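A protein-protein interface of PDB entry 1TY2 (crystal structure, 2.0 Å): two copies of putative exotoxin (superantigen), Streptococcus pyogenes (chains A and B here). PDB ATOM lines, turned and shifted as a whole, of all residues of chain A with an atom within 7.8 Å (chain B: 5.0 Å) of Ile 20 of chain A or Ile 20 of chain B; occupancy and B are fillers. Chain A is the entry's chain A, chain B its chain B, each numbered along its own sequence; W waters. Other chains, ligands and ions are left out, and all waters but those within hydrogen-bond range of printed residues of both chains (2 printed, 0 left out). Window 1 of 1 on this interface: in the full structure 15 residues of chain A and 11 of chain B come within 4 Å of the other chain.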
ATOM      1  N   LEU A  14      34.794  -4.896 -21.046  1.00  0.00           N
ATOM      2  CA  LEU A  14      33.541  -4.395 -21.578  1.00  0.00           C
ATOM      3  C   LEU A  14      32.357  -5.157 -20.999  1.00  0.00           C
ATOM      4  O   LEU A  14      31.310  -4.570 -20.728  1.00  0.00           O
ATOM      5  CB  LEU A  14      33.550  -4.497 -23.102  1.00  0.00           C
ATOM      6  CG  LEU A  14      34.430  -3.451 -23.802  1.00  0.00           C
ATOM      7  CD1 LEU A  14      34.856  -3.945 -25.187  1.00  0.00           C
ATOM      8  CD2 LEU A  14      33.661  -2.147 -23.900  1.00  0.00           C
ATOM      9  N   ASN A  15      32.530  -6.462 -20.805  1.00  0.00           N
ATOM     10  CA  ASN A  15      31.458  -7.279 -20.265  1.00  0.00           C
ATOM     11  C   ASN A  15      31.138  -6.813 -18.860  1.00  0.00           C
ATOM     12  O   ASN A  15      29.975  -6.636 -18.500  1.00  0.00           O
ATOM     13  CB  ASN A  15      31.856  -8.757 -20.252  1.00  0.00           C
ATOM     14  CG  ASN A  15      30.711  -9.651 -19.841  1.00  0.00           C
ATOM     15  OD1 ASN A  15      30.357  -9.725 -18.661  1.00  0.00           O
ATOM     16  ND2 ASN A  15      30.102 -10.319 -20.818  1.00  0.00           N
ATOM     17  N   TYR A  16      32.178  -6.604 -18.065  1.00  0.00           N
ATOM     18  CA  TYR A  16      31.994  -6.123 -16.702  1.00  0.00           C
ATOM     19  C   TYR A  16      31.405  -4.713 -16.696  1.00  0.00           C
ATOM     20  O   TYR A  16      30.473  -4.418 -15.948  1.00  0.00           O
ATOM     21  CB  TYR A  16      33.335  -6.090 -15.965  1.00  0.00           C
ATOM     22  CG  TYR A  16      33.436  -4.956 -14.966  1.00  0.00           C
ATOM     23  CD1 TYR A  16      32.702  -4.973 -13.775  1.00  0.00           C
ATOM     24  CD2 TYR A  16      34.224  -3.833 -15.240  1.00  0.00           C
ATOM     25  CE1 TYR A  16      32.748  -3.895 -12.883  1.00  0.00           C
ATOM     26  CE2 TYR A  16      34.277  -2.752 -14.358  1.00  0.00           C
ATOM     27  CZ  TYR A  16      33.535  -2.790 -13.185  1.00  0.00           C
ATOM     28  OH  TYR A  16      33.573  -1.714 -12.323  1.00  0.00           O
ATOM     29  N   ALA A  17      31.960  -3.841 -17.532  1.00  0.00           N
ATOM     30  CA  ALA A  17      31.516  -2.455 -17.573  1.00  0.00           C
ATOM     31  C   ALA A  17      30.018  -2.311 -17.802  1.00  0.00           C
ATOM     32  O   ALA A  17      29.340  -1.581 -17.076  1.00  0.00           O
ATOM     33  CB  ALA A  17      32.297  -1.680 -18.661  1.00  0.00           C
ATOM     34  N   TYR A  18      29.508  -3.032 -18.797  1.00  0.00           N
ATOM     35  CA  TYR A  18      28.103  -2.955 -19.164  1.00  0.00           C
ATOM     36  C   TYR A  18      27.094  -3.860 -18.448  1.00  0.00           C
ATOM     37  O   TYR A  18      25.906  -3.817 -18.768  1.00  0.00           O
ATOM     38  CB  TYR A  18      27.978  -3.102 -20.687  1.00  0.00           C
ATOM     39  CG  TYR A  18      28.398  -1.846 -21.441  1.00  0.00           C
ATOM     40  CD1 TYR A  18      27.515  -0.775 -21.588  1.00  0.00           C
ATOM     41  CD2 TYR A  18      29.681  -1.720 -21.983  1.00  0.00           C
ATOM     42  CE1 TYR A  18      27.888   0.390 -22.254  1.00  0.00           C
ATOM     43  CE2 TYR A  18      30.073  -0.554 -22.649  1.00  0.00           C
ATOM     44  CZ  TYR A  18      29.169   0.498 -22.781  1.00  0.00           C
ATOM     45  OH  TYR A  18      29.532   1.656 -23.432  1.00  0.00           O
ATOM     46  N   GLU A  19      27.543  -4.689 -17.508  1.00  0.00           N
ATOM     47  CA  GLU A  19      26.596  -5.509 -16.743  1.00  0.00           C
ATOM     48  C   GLU A  19      26.317  -4.633 -15.528  1.00  0.00           C
ATOM     49  O   GLU A  19      26.888  -4.821 -14.456  1.00  0.00           O
ATOM     50  CB  GLU A  19      27.203  -6.852 -16.304  1.00  0.00           C
ATOM     51  CG  GLU A  19      27.420  -7.852 -17.442  1.00  0.00           C
ATOM     52  CD  GLU A  19      27.287  -9.308 -16.993  1.00  0.00           C
ATOM     53  OE1 GLU A  19      27.702  -9.637 -15.859  1.00  0.00           O
ATOM     54  OE2 GLU A  19      26.777 -10.130 -17.787  1.00  0.00           O
ATOM     55  N   ILE A  20      25.434  -3.659 -15.713  1.00  0.00           N
ATOM     56  CA  ILE A  20      25.122  -2.707 -14.659  1.00  0.00           C
ATOM     57  C   ILE A  20      23.681  -2.218 -14.718  1.00  0.00           C
ATOM     58  O   ILE A  20      23.040  -2.263 -15.765  1.00  0.00           O
ATOM     59  CB  ILE A  20      26.057  -1.490 -14.798  1.00  0.00           C
ATOM     60  CG1 ILE A  20      25.789  -0.458 -13.708  1.00  0.00           C
ATOM     61  CG2 ILE A  20      25.845  -0.848 -16.166  1.00  0.00           C
ATOM     62  CD1 ILE A  20      26.710   0.737 -13.814  1.00  0.00           C
ATOM     63  N   ILE A  21      23.178  -1.748 -13.587  1.00  0.00           N
ATOM     64  CA  ILE A  21      21.827  -1.215 -13.520  1.00  0.00           C
ATOM     65  C   ILE A  21      21.975   0.280 -13.782  1.00  0.00           C
ATOM     66  O   ILE A  21      22.757   0.961 -13.117  1.00  0.00           O
ATOM     67  CB  ILE A  21      21.203  -1.429 -12.132  1.00  0.00           C
ATOM     68  CG1 ILE A  21      21.132  -2.927 -11.820  1.00  0.00           C
ATOM     69  CG2 ILE A  21      19.816  -0.822 -12.088  1.00  0.00           C
ATOM     70  CD1 ILE A  21      20.213  -3.707 -12.731  1.00  0.00           C
ATOM     71  N   PRO A  22      21.246   0.802 -14.774  1.00  0.00           N
ATOM     72  CA  PRO A  22      21.314   2.225 -15.111  1.00  0.00           C
ATOM     73  C   PRO A  22      20.540   3.137 -14.180  1.00  0.00           C
ATOM     74  O   PRO A  22      19.719   2.681 -13.387  1.00  0.00           O
ATOM     75  CB  PRO A  22      20.746   2.265 -16.529  1.00  0.00           C
ATOM     76  CG  PRO A  22      19.699   1.206 -16.481  1.00  0.00           C
ATOM     77  CD  PRO A  22      20.399   0.076 -15.740  1.00  0.00           C
ATOM     78  N   VAL A  23      20.836   4.432 -14.287  1.00  0.00           N
ATOM     79  CA  VAL A  23      20.155   5.477 -13.528  1.00  0.00           C
ATOM     80  C   VAL A  23      19.071   5.892 -14.511  1.00  0.00           C
ATOM     81  O   VAL A  23      19.356   6.475 -15.559  1.00  0.00           O
ATOM     82  CB  VAL A  23      21.099   6.668 -13.241  1.00  0.00           C
ATOM     83  CG1 VAL A  23      20.320   7.814 -12.622  1.00  0.00           C
ATOM     84  CG2 VAL A  23      22.217   6.226 -12.308  1.00  0.00           C
ATOM     85  N   PHE A  73      18.883   8.954 -18.218  1.00  0.00           N
ATOM     86  CA  PHE A  73      19.250   7.572 -18.497  1.00  0.00           C
ATOM     87  C   PHE A  73      20.756   7.581 -18.686  1.00  0.00           C
ATOM     88  O   PHE A  73      21.266   7.958 -19.742  1.00  0.00           O
ATOM     89  CB  PHE A  73      18.569   6.996 -19.745  1.00  0.00           C
ATOM     90  CG  PHE A  73      18.584   5.481 -19.780  1.00  0.00           C
ATOM     91  CD1 PHE A  73      17.431   4.750 -19.497  1.00  0.00           C
ATOM     92  CD2 PHE A  73      19.769   4.791 -20.037  1.00  0.00           C
ATOM     93  CE1 PHE A  73      17.456   3.340 -19.469  1.00  0.00           C
ATOM     94  CE2 PHE A  73      19.809   3.384 -20.012  1.00  0.00           C
ATOM     95  CZ  PHE A  73      18.653   2.662 -19.727  1.00  0.00           C
ATOM     96  N   GLY A  74      21.459   7.177 -17.636  1.00  0.00           N
ATOM     97  CA  GLY A  74      22.905   7.162 -17.676  1.00  0.00           C
ATOM     98  C   GLY A  74      23.477   6.029 -16.858  1.00  0.00           C
ATOM     99  O   GLY A  74      22.847   5.525 -15.926  1.00  0.00           O
ATOM    100  N   LEU A  75      24.683   5.617 -17.213  1.00  0.00           N
ATOM    101  CA  LEU A  75      25.334   4.528 -16.500  1.00  0.00           C
ATOM    102  C   LEU A  75      26.267   5.135 -15.461  1.00  0.00           C
ATOM    103  O   LEU A  75      27.157   5.917 -15.799  1.00  0.00           O
ATOM    104  CB  LEU A  75      26.117   3.662 -17.487  1.00  0.00           C
ATOM    105  CG  LEU A  75      25.346   3.299 -18.763  1.00  0.00           C
ATOM    106  CD1 LEU A  75      26.216   2.453 -19.674  1.00  0.00           C
ATOM    107  CD2 LEU A  75      24.059   2.557 -18.398  1.00  0.00           C
ATOM    108  N   PRO A  76      26.073   4.787 -14.182  1.00  0.00           N
ATOM    109  CA  PRO A  76      26.932   5.334 -13.127  1.00  0.00           C
ATOM    110  C   PRO A  76      28.380   4.898 -13.322  1.00  0.00           C
ATOM    111  O   PRO A  76      28.640   3.738 -13.608  1.00  0.00           O
ATOM    112  CB  PRO A  76      26.308   4.773 -11.852  1.00  0.00           C
ATOM    113  CG  PRO A  76      25.784   3.440 -12.301  1.00  0.00           C
ATOM    114  CD  PRO A  76      25.138   3.782 -13.634  1.00  0.00           C
ATOM    115  N   TYR A  77      29.315   5.831 -13.180  1.00  0.00           N
ATOM    116  CA  TYR A  77      30.724   5.503 -13.369  1.00  0.00           C
ATOM    117  C   TYR A  77      31.510   5.428 -12.067  1.00  0.00           C
ATOM    118  O   TYR A  77      32.630   4.933 -12.046  1.00  0.00           O
ATOM    119  CB  TYR A  77      31.385   6.501 -14.341  1.00  0.00           C
ATOM    120  CG  TYR A  77      31.401   7.953 -13.889  1.00  0.00           C
ATOM    121  CD1 TYR A  77      32.410   8.434 -13.052  1.00  0.00           C
ATOM    122  CD2 TYR A  77      30.414   8.844 -14.313  1.00  0.00           C
ATOM    123  CE1 TYR A  77      32.439   9.766 -12.654  1.00  0.00           C
ATOM    124  CE2 TYR A  77      30.428  10.176 -13.921  1.00  0.00           C
ATOM    125  CZ  TYR A  77      31.446  10.633 -13.094  1.00  0.00           C
ATOM    126  OH  TYR A  77      31.472  11.953 -12.719  1.00  0.00           O
ATOM    127  N   ILE A  78      30.920   5.907 -10.981  1.00  0.00           N
ATOM    128  CA  ILE A  78      31.587   5.861  -9.685  1.00  0.00           C
ATOM    129  C   ILE A  78      30.564   5.997  -8.571  1.00  0.00           C
ATOM    130  O   ILE A  78      29.501   6.577  -8.779  1.00  0.00           O
ATOM    131  CB  ILE A  78      32.644   6.995  -9.554  1.00  0.00           C
ATOM    132  CG1 ILE A  78      33.589   6.681  -8.399  1.00  0.00           C
ATOM    133  CG2 ILE A  78      31.966   8.352  -9.297  1.00  0.00           C
ATOM    134  CD1 ILE A  78      34.317   5.359  -8.554  1.00  0.00           C
ATOM    135  N   PHE A  79      30.864   5.429  -7.402  1.00  0.00           N
ATOM    136  CA  PHE A  79      29.963   5.538  -6.250  1.00  0.00           C
ATOM    137  C   PHE A  79      30.694   6.232  -5.112  1.00  0.00           C
ATOM    138  O   PHE A  79      31.907   6.084  -4.963  1.00  0.00           O
ATOM    139  CB  PHE A  79      29.487   4.167  -5.769  1.00  0.00           C
ATOM    140  CG  PHE A  79      28.640   3.433  -6.768  1.00  0.00           C
ATOM    141  CD1 PHE A  79      27.498   4.028  -7.302  1.00  0.00           C
ATOM    142  CD2 PHE A  79      28.979   2.145  -7.171  1.00  0.00           C
ATOM    143  CE1 PHE A  79      26.705   3.353  -8.228  1.00  0.00           C
ATOM    144  CE2 PHE A  79      28.190   1.456  -8.099  1.00  0.00           C
ATOM    145  CZ  PHE A  79      27.054   2.064  -8.626  1.00  0.00           C
ATOM    146  N   PHE A 136      23.611   1.281 -24.551  1.00  0.00           N
ATOM    147  CA  PHE A 136      23.512   0.402 -23.396  1.00  0.00           C
ATOM    148  C   PHE A 136      22.563  -0.769 -23.622  1.00  0.00           C
ATOM    149  O   PHE A 136      22.914  -1.921 -23.382  1.00  0.00           O
ATOM    150  CB  PHE A 136      23.006   1.165 -22.170  1.00  0.00           C
ATOM    151  CG  PHE A 136      22.643   0.269 -21.023  1.00  0.00           C
ATOM    152  CD1 PHE A 136      23.630  -0.419 -20.323  1.00  0.00           C
ATOM    153  CD2 PHE A 136      21.312   0.060 -20.677  1.00  0.00           C
ATOM    154  CE1 PHE A 136      23.298  -1.310 -19.292  1.00  0.00           C
ATOM    155  CE2 PHE A 136      20.973  -0.823 -19.654  1.00  0.00           C
ATOM    156  CZ  PHE A 136      21.972  -1.513 -18.958  1.00  0.00           C
ATOM    157  N   GLN A 140      23.526  -4.745 -24.141  1.00  0.00           N
ATOM    158  CA  GLN A 140      22.990  -5.767 -23.250  1.00  0.00           C
ATOM    159  C   GLN A 140      22.342  -6.860 -24.103  1.00  0.00           C
ATOM    160  O   GLN A 140      22.575  -8.054 -23.893  1.00  0.00           O
ATOM    161  CB  GLN A 140      21.954  -5.171 -22.291  1.00  0.00           C
ATOM    162  CG  GLN A 140      22.509  -4.744 -20.941  1.00  0.00           C
ATOM    163  CD  GLN A 140      23.082  -5.908 -20.152  1.00  0.00           C
ATOM    164  OE1 GLN A 140      22.479  -6.984 -20.080  1.00  0.00           O
ATOM    165  NE2 GLN A 140      24.245  -5.698 -19.543  1.00  0.00           N
ATOM    166  N   MET A 143      24.913  -8.855 -25.734  1.00  0.00           N
ATOM    167  CA  MET A 143      25.617  -9.648 -24.737  1.00  0.00           C
ATOM    168  C   MET A 143      24.824 -10.913 -24.405  1.00  0.00           C
ATOM    169  O   MET A 143      25.355 -12.021 -24.447  1.00  0.00           O
ATOM    170  CB  MET A 143      25.842  -8.809 -23.469  1.00  0.00           C
ATOM    171  CG  MET A 143      26.913  -7.729 -23.634  1.00  0.00           C
ATOM    172  SD  MET A 143      26.867  -6.390 -22.410  1.00  0.00           S
ATOM    173  CE  MET A 143      27.477  -7.219 -20.937  1.00  0.00           C
ATOM    174  N   ARG A 183      35.114   1.747 -15.818  1.00  0.00           N
ATOM    175  CA  ARG A 183      33.814   2.222 -16.272  1.00  0.00           C
ATOM    176  C   ARG A 183      33.897   3.686 -16.660  1.00  0.00           C
ATOM    177  O   ARG A 183      33.339   4.101 -17.678  1.00  0.00           O
ATOM    178  CB  ARG A 183      32.756   2.020 -15.188  1.00  0.00           C
ATOM    179  CG  ARG A 183      32.015   0.718 -15.347  1.00  0.00           C
ATOM    180  CD  ARG A 183      31.008   0.490 -14.246  1.00  0.00           C
ATOM    181  NE  ARG A 183      30.278  -0.744 -14.500  1.00  0.00           N
ATOM    182  CZ  ARG A 183      29.803  -1.543 -13.556  1.00  0.00           C
ATOM    183  NH1 ARG A 183      29.978  -1.239 -12.271  1.00  0.00           N
ATOM    184  NH2 ARG A 183      29.175  -2.660 -13.901  1.00  0.00           N
ATOM    185  N   PHE A 187      32.726   4.887 -20.195  1.00  0.00           N
ATOM    186  CA  PHE A 187      31.530   5.712 -20.288  1.00  0.00           C
ATOM    187  C   PHE A 187      31.766   7.184 -20.611  1.00  0.00           C
ATOM    188  O   PHE A 187      30.826   7.886 -20.968  1.00  0.00           O
ATOM    189  CB  PHE A 187      30.711   5.639 -18.987  1.00  0.00           C
ATOM    190  CG  PHE A 187      30.253   4.245 -18.614  1.00  0.00           C
ATOM    191  CD1 PHE A 187      30.276   3.203 -19.542  1.00  0.00           C
ATOM    192  CD2 PHE A 187      29.773   3.989 -17.331  1.00  0.00           C
ATOM    193  CE1 PHE A 187      29.830   1.930 -19.196  1.00  0.00           C
ATOM    194  CE2 PHE A 187      29.321   2.716 -16.972  1.00  0.00           C
ATOM    195  CZ  PHE A 187      29.348   1.687 -17.903  1.00  0.00           C
ATOM    196  N   ALA B  17      31.757  -7.926  -8.766  1.00  0.00           N
ATOM    197  CA  ALA B  17      30.464  -8.258  -8.186  1.00  0.00           C
ATOM    198  C   ALA B  17      29.743  -7.176  -7.388  1.00  0.00           C
ATOM    199  O   ALA B  17      28.555  -6.933  -7.596  1.00  0.00           O
ATOM    200  CB  ALA B  17      30.607  -9.530  -7.333  1.00  0.00           C
ATOM    201  N   TYR B  18      30.454  -6.508  -6.487  1.00  0.00           N
ATOM    202  CA  TYR B  18      29.814  -5.512  -5.644  1.00  0.00           C
ATOM    203  C   TYR B  18      29.705  -4.075  -6.163  1.00  0.00           C
ATOM    204  O   TYR B  18      29.048  -3.245  -5.543  1.00  0.00           O
ATOM    205  CB  TYR B  18      30.462  -5.559  -4.246  1.00  0.00           C
ATOM    206  CG  TYR B  18      30.030  -6.782  -3.437  1.00  0.00           C
ATOM    207  CD1 TYR B  18      28.789  -6.809  -2.790  1.00  0.00           C
ATOM    208  CD2 TYR B  18      30.846  -7.911  -3.336  1.00  0.00           C
ATOM    209  CE1 TYR B  18      28.369  -7.926  -2.064  1.00  0.00           C
ATOM    210  CE2 TYR B  18      30.429  -9.051  -2.598  1.00  0.00           C
ATOM    211  CZ  TYR B  18      29.192  -9.042  -1.969  1.00  0.00           C
ATOM    212  OH  TYR B  18      28.770 -10.132  -1.222  1.00  0.00           O
ATOM    213  N   GLU B  19      30.333  -3.780  -7.296  1.00  0.00           N
ATOM    214  CA  GLU B  19      30.249  -2.440  -7.881  1.00  0.00           C
ATOM    215  C   GLU B  19      28.976  -2.482  -8.733  1.00  0.00           C
ATOM    216  O   GLU B  19      29.041  -2.667  -9.949  1.00  0.00           O
ATOM    217  CB  GLU B  19      31.472  -2.178  -8.776  1.00  0.00           C
ATOM    218  CG  GLU B  19      31.631  -0.719  -9.223  1.00  0.00           C
ATOM    219  CD  GLU B  19      32.076   0.190  -8.092  1.00  0.00           C
ATOM    220  OE1 GLU B  19      32.255  -0.312  -6.963  1.00  0.00           O
ATOM    221  OE2 GLU B  19      32.246   1.403  -8.329  1.00  0.00           O
ATOM    222  N   ILE B  20      27.823  -2.307  -8.093  1.00  0.00           N
ATOM    223  CA  ILE B  20      26.550  -2.396  -8.791  1.00  0.00           C
ATOM    224  C   ILE B  20      25.454  -1.616  -8.071  1.00  0.00           C
ATOM    225  O   ILE B  20      25.550  -1.359  -6.869  1.00  0.00           O
ATOM    226  CB  ILE B  20      26.114  -3.897  -8.887  1.00  0.00           C
ATOM    227  CG1 ILE B  20      24.782  -4.044  -9.629  1.00  0.00           C
ATOM    228  CG2 ILE B  20      25.963  -4.475  -7.475  1.00  0.00           C
ATOM    229  CD1 ILE B  20      24.807  -3.558 -11.075  1.00  0.00           C
ATOM    230  N   ILE B  21      24.420  -1.214  -8.804  1.00  0.00           N
ATOM    231  CA  ILE B  21      23.312  -0.534  -8.158  1.00  0.00           C
ATOM    232  C   ILE B  21      22.392  -1.660  -7.687  1.00  0.00           C
ATOM    233  O   ILE B  21      22.144  -2.623  -8.413  1.00  0.00           O
ATOM    234  CB  ILE B  21      22.562   0.427  -9.121  1.00  0.00           C
ATOM    235  CG1 ILE B  21      23.345   1.743  -9.235  1.00  0.00           C
ATOM    236  CG2 ILE B  21      21.157   0.714  -8.599  1.00  0.00           C
ATOM    237  CD1 ILE B  21      22.674   2.811 -10.079  1.00  0.00           C
ATOM    238  N   PRO B  22      21.909  -1.574  -6.445  1.00  0.00           N
ATOM    239  CA  PRO B  22      21.026  -2.615  -5.913  1.00  0.00           C
ATOM    240  C   PRO B  22      19.559  -2.469  -6.311  1.00  0.00           C
ATOM    241  O   PRO B  22      19.104  -1.380  -6.674  1.00  0.00           O
ATOM    242  CB  PRO B  22      21.209  -2.471  -4.410  1.00  0.00           C
ATOM    243  CG  PRO B  22      21.344  -0.980  -4.263  1.00  0.00           C
ATOM    244  CD  PRO B  22      22.319  -0.642  -5.379  1.00  0.00           C
ATOM    245  N   LEU B  75      21.010  -7.793  -4.584  1.00  0.00           N
ATOM    246  CA  LEU B  75      21.965  -7.512  -5.632  1.00  0.00           C
ATOM    247  C   LEU B  75      21.681  -8.425  -6.823  1.00  0.00           C
ATOM    248  O   LEU B  75      21.676  -9.657  -6.692  1.00  0.00           O
ATOM    249  CB  LEU B  75      23.382  -7.737  -5.106  1.00  0.00           C
ATOM    250  CG  LEU B  75      23.664  -7.047  -3.760  1.00  0.00           C
ATOM    251  CD1 LEU B  75      25.110  -7.295  -3.370  1.00  0.00           C
ATOM    252  CD2 LEU B  75      23.387  -5.540  -3.862  1.00  0.00           C
ATOM    253  N   PRO B  76      21.437  -7.834  -8.002  1.00  0.00           N
ATOM    254  CA  PRO B  76      21.158  -8.637  -9.196  1.00  0.00           C
ATOM    255  C   PRO B  76      22.375  -9.485  -9.570  1.00  0.00           C
ATOM    256  O   PRO B  76      23.501  -8.981  -9.613  1.00  0.00           O
ATOM    257  CB  PRO B  76      20.814  -7.577 -10.248  1.00  0.00           C
ATOM    258  CG  PRO B  76      21.659  -6.394  -9.814  1.00  0.00           C
ATOM    259  CD  PRO B  76      21.434  -6.390  -8.320  1.00  0.00           C
ATOM    260  N   PHE B  79      21.649 -10.540 -15.807  1.00  0.00           N
ATOM    261  CA  PHE B  79      20.825  -9.621 -16.592  1.00  0.00           C
ATOM    262  C   PHE B  79      20.257 -10.317 -17.831  1.00  0.00           C
ATOM    263  O   PHE B  79      20.972 -11.016 -18.546  1.00  0.00           O
ATOM    264  CB  PHE B  79      21.667  -8.409 -16.997  1.00  0.00           C
ATOM    265  CG  PHE B  79      22.337  -7.726 -15.832  1.00  0.00           C
ATOM    266  CD1 PHE B  79      21.608  -6.902 -14.977  1.00  0.00           C
ATOM    267  CD2 PHE B  79      23.688  -7.949 -15.560  1.00  0.00           C
ATOM    268  CE1 PHE B  79      22.214  -6.309 -13.865  1.00  0.00           C
ATOM    269  CE2 PHE B  79      24.301  -7.362 -14.451  1.00  0.00           C
ATOM    270  CZ  PHE B  79      23.560  -6.539 -13.601  1.00  0.00           C
ATOM    271  N   PHE B 136      26.296  -5.374   1.860  1.00  0.00           N
ATOM    272  CA  PHE B 136      26.507  -4.598   0.649  1.00  0.00           C
ATOM    273  C   PHE B 136      27.023  -3.194   0.959  1.00  0.00           C
ATOM    274  O   PHE B 136      28.037  -2.767   0.421  1.00  0.00           O
ATOM    275  CB  PHE B 136      25.205  -4.466  -0.144  1.00  0.00           C
ATOM    276  CG  PHE B 136      25.287  -3.464  -1.274  1.00  0.00           C
ATOM    277  CD1 PHE B 136      26.031  -3.745  -2.416  1.00  0.00           C
ATOM    278  CD2 PHE B 136      24.659  -2.224  -1.171  1.00  0.00           C
ATOM    279  CE1 PHE B 136      26.153  -2.800  -3.448  1.00  0.00           C
ATOM    280  CE2 PHE B 136      24.774  -1.274  -2.191  1.00  0.00           C
ATOM    281  CZ  PHE B 136      25.523  -1.564  -3.330  1.00  0.00           C
ATOM    282  N   GLN B 140      30.683  -1.563   0.084  1.00  0.00           N
ATOM    283  CA  GLN B 140      30.802  -0.381  -0.766  1.00  0.00           C
ATOM    284  C   GLN B 140      31.584   0.688  -0.012  1.00  0.00           C
ATOM    285  O   GLN B 140      32.420   1.380  -0.598  1.00  0.00           O
ATOM    286  CB  GLN B 140      29.426   0.152  -1.164  1.00  0.00           C
ATOM    287  CG  GLN B 140      28.979  -0.316  -2.545  1.00  0.00           C
ATOM    288  CD  GLN B 140      29.901   0.194  -3.642  1.00  0.00           C
ATOM    289  OE1 GLN B 140      30.425   1.311  -3.556  1.00  0.00           O
ATOM    290  NE2 GLN B 140      30.092  -0.612  -4.684  1.00  0.00           N
ATOM    291  N   ARG B 183      29.126 -13.551 -10.152  1.00  0.00           N
ATOM    292  CA  ARG B 183      28.291 -12.795  -9.236  1.00  0.00           C
ATOM    293  C   ARG B 183      27.321 -13.740  -8.550  1.00  0.00           C
ATOM    294  O   ARG B 183      27.063 -13.611  -7.359  1.00  0.00           O
ATOM    295  CB  ARG B 183      27.510 -11.723  -9.995  1.00  0.00           C
ATOM    296  CG  ARG B 183      28.230 -10.399 -10.041  1.00  0.00           C
ATOM    297  CD  ARG B 183      27.466  -9.353 -10.822  1.00  0.00           C
ATOM    298  NE  ARG B 183      28.042  -8.038 -10.571  1.00  0.00           N
ATOM    299  CZ  ARG B 183      27.797  -6.948 -11.287  1.00  0.00           C
ATOM    300  NH1 ARG B 183      26.979  -6.998 -12.327  1.00  0.00           N
ATOM    301  NH2 ARG B 183      28.369  -5.801 -10.948  1.00  0.00           N
HETATM  302  O   HOH W   1      32.485   1.918 -11.311  1.00  0.00           O
HETATM  303  O   HOH W   2      27.404  -0.003 -10.976  1.00  0.00           O
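The backbone carbonyl oxygen (O) of Tyr 16 of chain A sits at hydrogen-bond distance from the guanidinium group (NH2) of Arg 183 of chain A.
The guanidinium group (NE) of Arg 183 of chain A sits at hydrogen-bond distance from the backbone carbonyl oxygen (O) of Ala 17 of chain A (2.9 Å).
The backbone carbonyl oxygen (O) of Glu 19 of chain A is in hydrogen-bond range of the guanidinium group (NH2) of Arg 183 of chain A (3.2 Å).
O of Tyr 18 of chain B sits at hydrogen-bond distance from NE2 of Gln 140 of chain B, 3.0 Å away.
OE1 of Glu 19 of chain B is in hydrogen-bond range of NE2 of Gln 140 of chain B (3.2 Å).
The backbone carbonyl oxygen (O) of Glu 19 of chain B lies within hydrogen-bond range of the guanidinium group (NH2) of Arg 183 of chain B, at 3.4 Å.
Printed residues of chain B within 4 Å of Ile 20 of chain A: Ile 20 (3.7 Å).
Ile 20 of chain B touches just these residues of chain A: Ile 20, Ile 21 and Phe 79.
Printed residues of chain A within 4 Å of Glu 19 of chain B: Tyr 16 (3.8 Å), Phe 79 (3.5 Å) and Arg 183 (2.9 Å).
Printed residues of chain B within 4 Å of Ile 21 of chain A: Ile 20, Ile 21 and Phe 79.
The nearest residue of chain A that does not touch Ile 20 of chain B is Glu 19 of chain A (4.2 Å).
Glu 19 of chain B touches Tyr 16 of chain A.
Phe 79 of chain B touches Glu 19 of chain A.
Ile 20 of chain A touches Ile 20 of chain B (CA to CD1, 3.7 Å).
N of Ile 21 of chain A touches CD1 of Ile 20 of chain B, 3.5 Å away.
Ile 21 of chain A touches Ile 21 of chain B.
Ile 21 of chain A touches Phe 79 of chain B.
Pro 76 of chain A touches Ile 21 of chain B (CG to CD1, 3.9 Å).
Phe 79 of chain A touches Ile 20 of chain B.
CZ of Phe 79 of chain A touches CG1 of Ile 21 of chain B (3.8 Å).
Phe 79 of chain A touches Gln 140 of chain B.
The guanidinium group (NH1) of Arg 183 of chain B is in hydrogen-bond range of the backbone carbonyl oxygen (O) of Glu 19 of chain A (3.0 Å).
NH1 of Arg 183 of chain A lies within hydrogen-bond range of O of Glu 19 of chain B (2.9 Å).
Of the 12 printed residues of chain B, 6 touch a printed residue of chain A.
Hydrophobic or aromatic side chains of chain B that line the printed part of chain A: Ile 20, Ile 21 and Phe 79.
Glu 19 of chain A touches Arg 183 of chain B, and with the chains exchanged Arg 183 of chain A touches Glu 19 of chain B.
Ile 21 of chain A touches Ile 20 of chain B, but with the chains exchanged Ile 20 of chain A does not touch Ile 21 of chain B (5.1 Å).
Phe 79 of chain A touches Ile 20 of chain B, but with the chains exchanged Ile 20 of chain A does not touch Phe 79 of chain B (4.03 Å).
Phe 79 of chain A touches Gln 140 of chain B, and with the chains exchanged Gln 140 of chain A touches Phe 79 of chain B.
12 positions are printed for both chains.
Of the 14 pairs that touch across the chains among the printed residues, 10 have their exchanged pair printed and touching as well.
Water W1 lies within hydrogen-bond range of OE2 of Glu 19 of chain B and O of Tyr 77 of chain A.
Water W2 lies within hydrogen-bond range of NH1 of Arg 183 of chain A (3.1 Å) and O of Glu 19 of chain B (3.3 Å).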
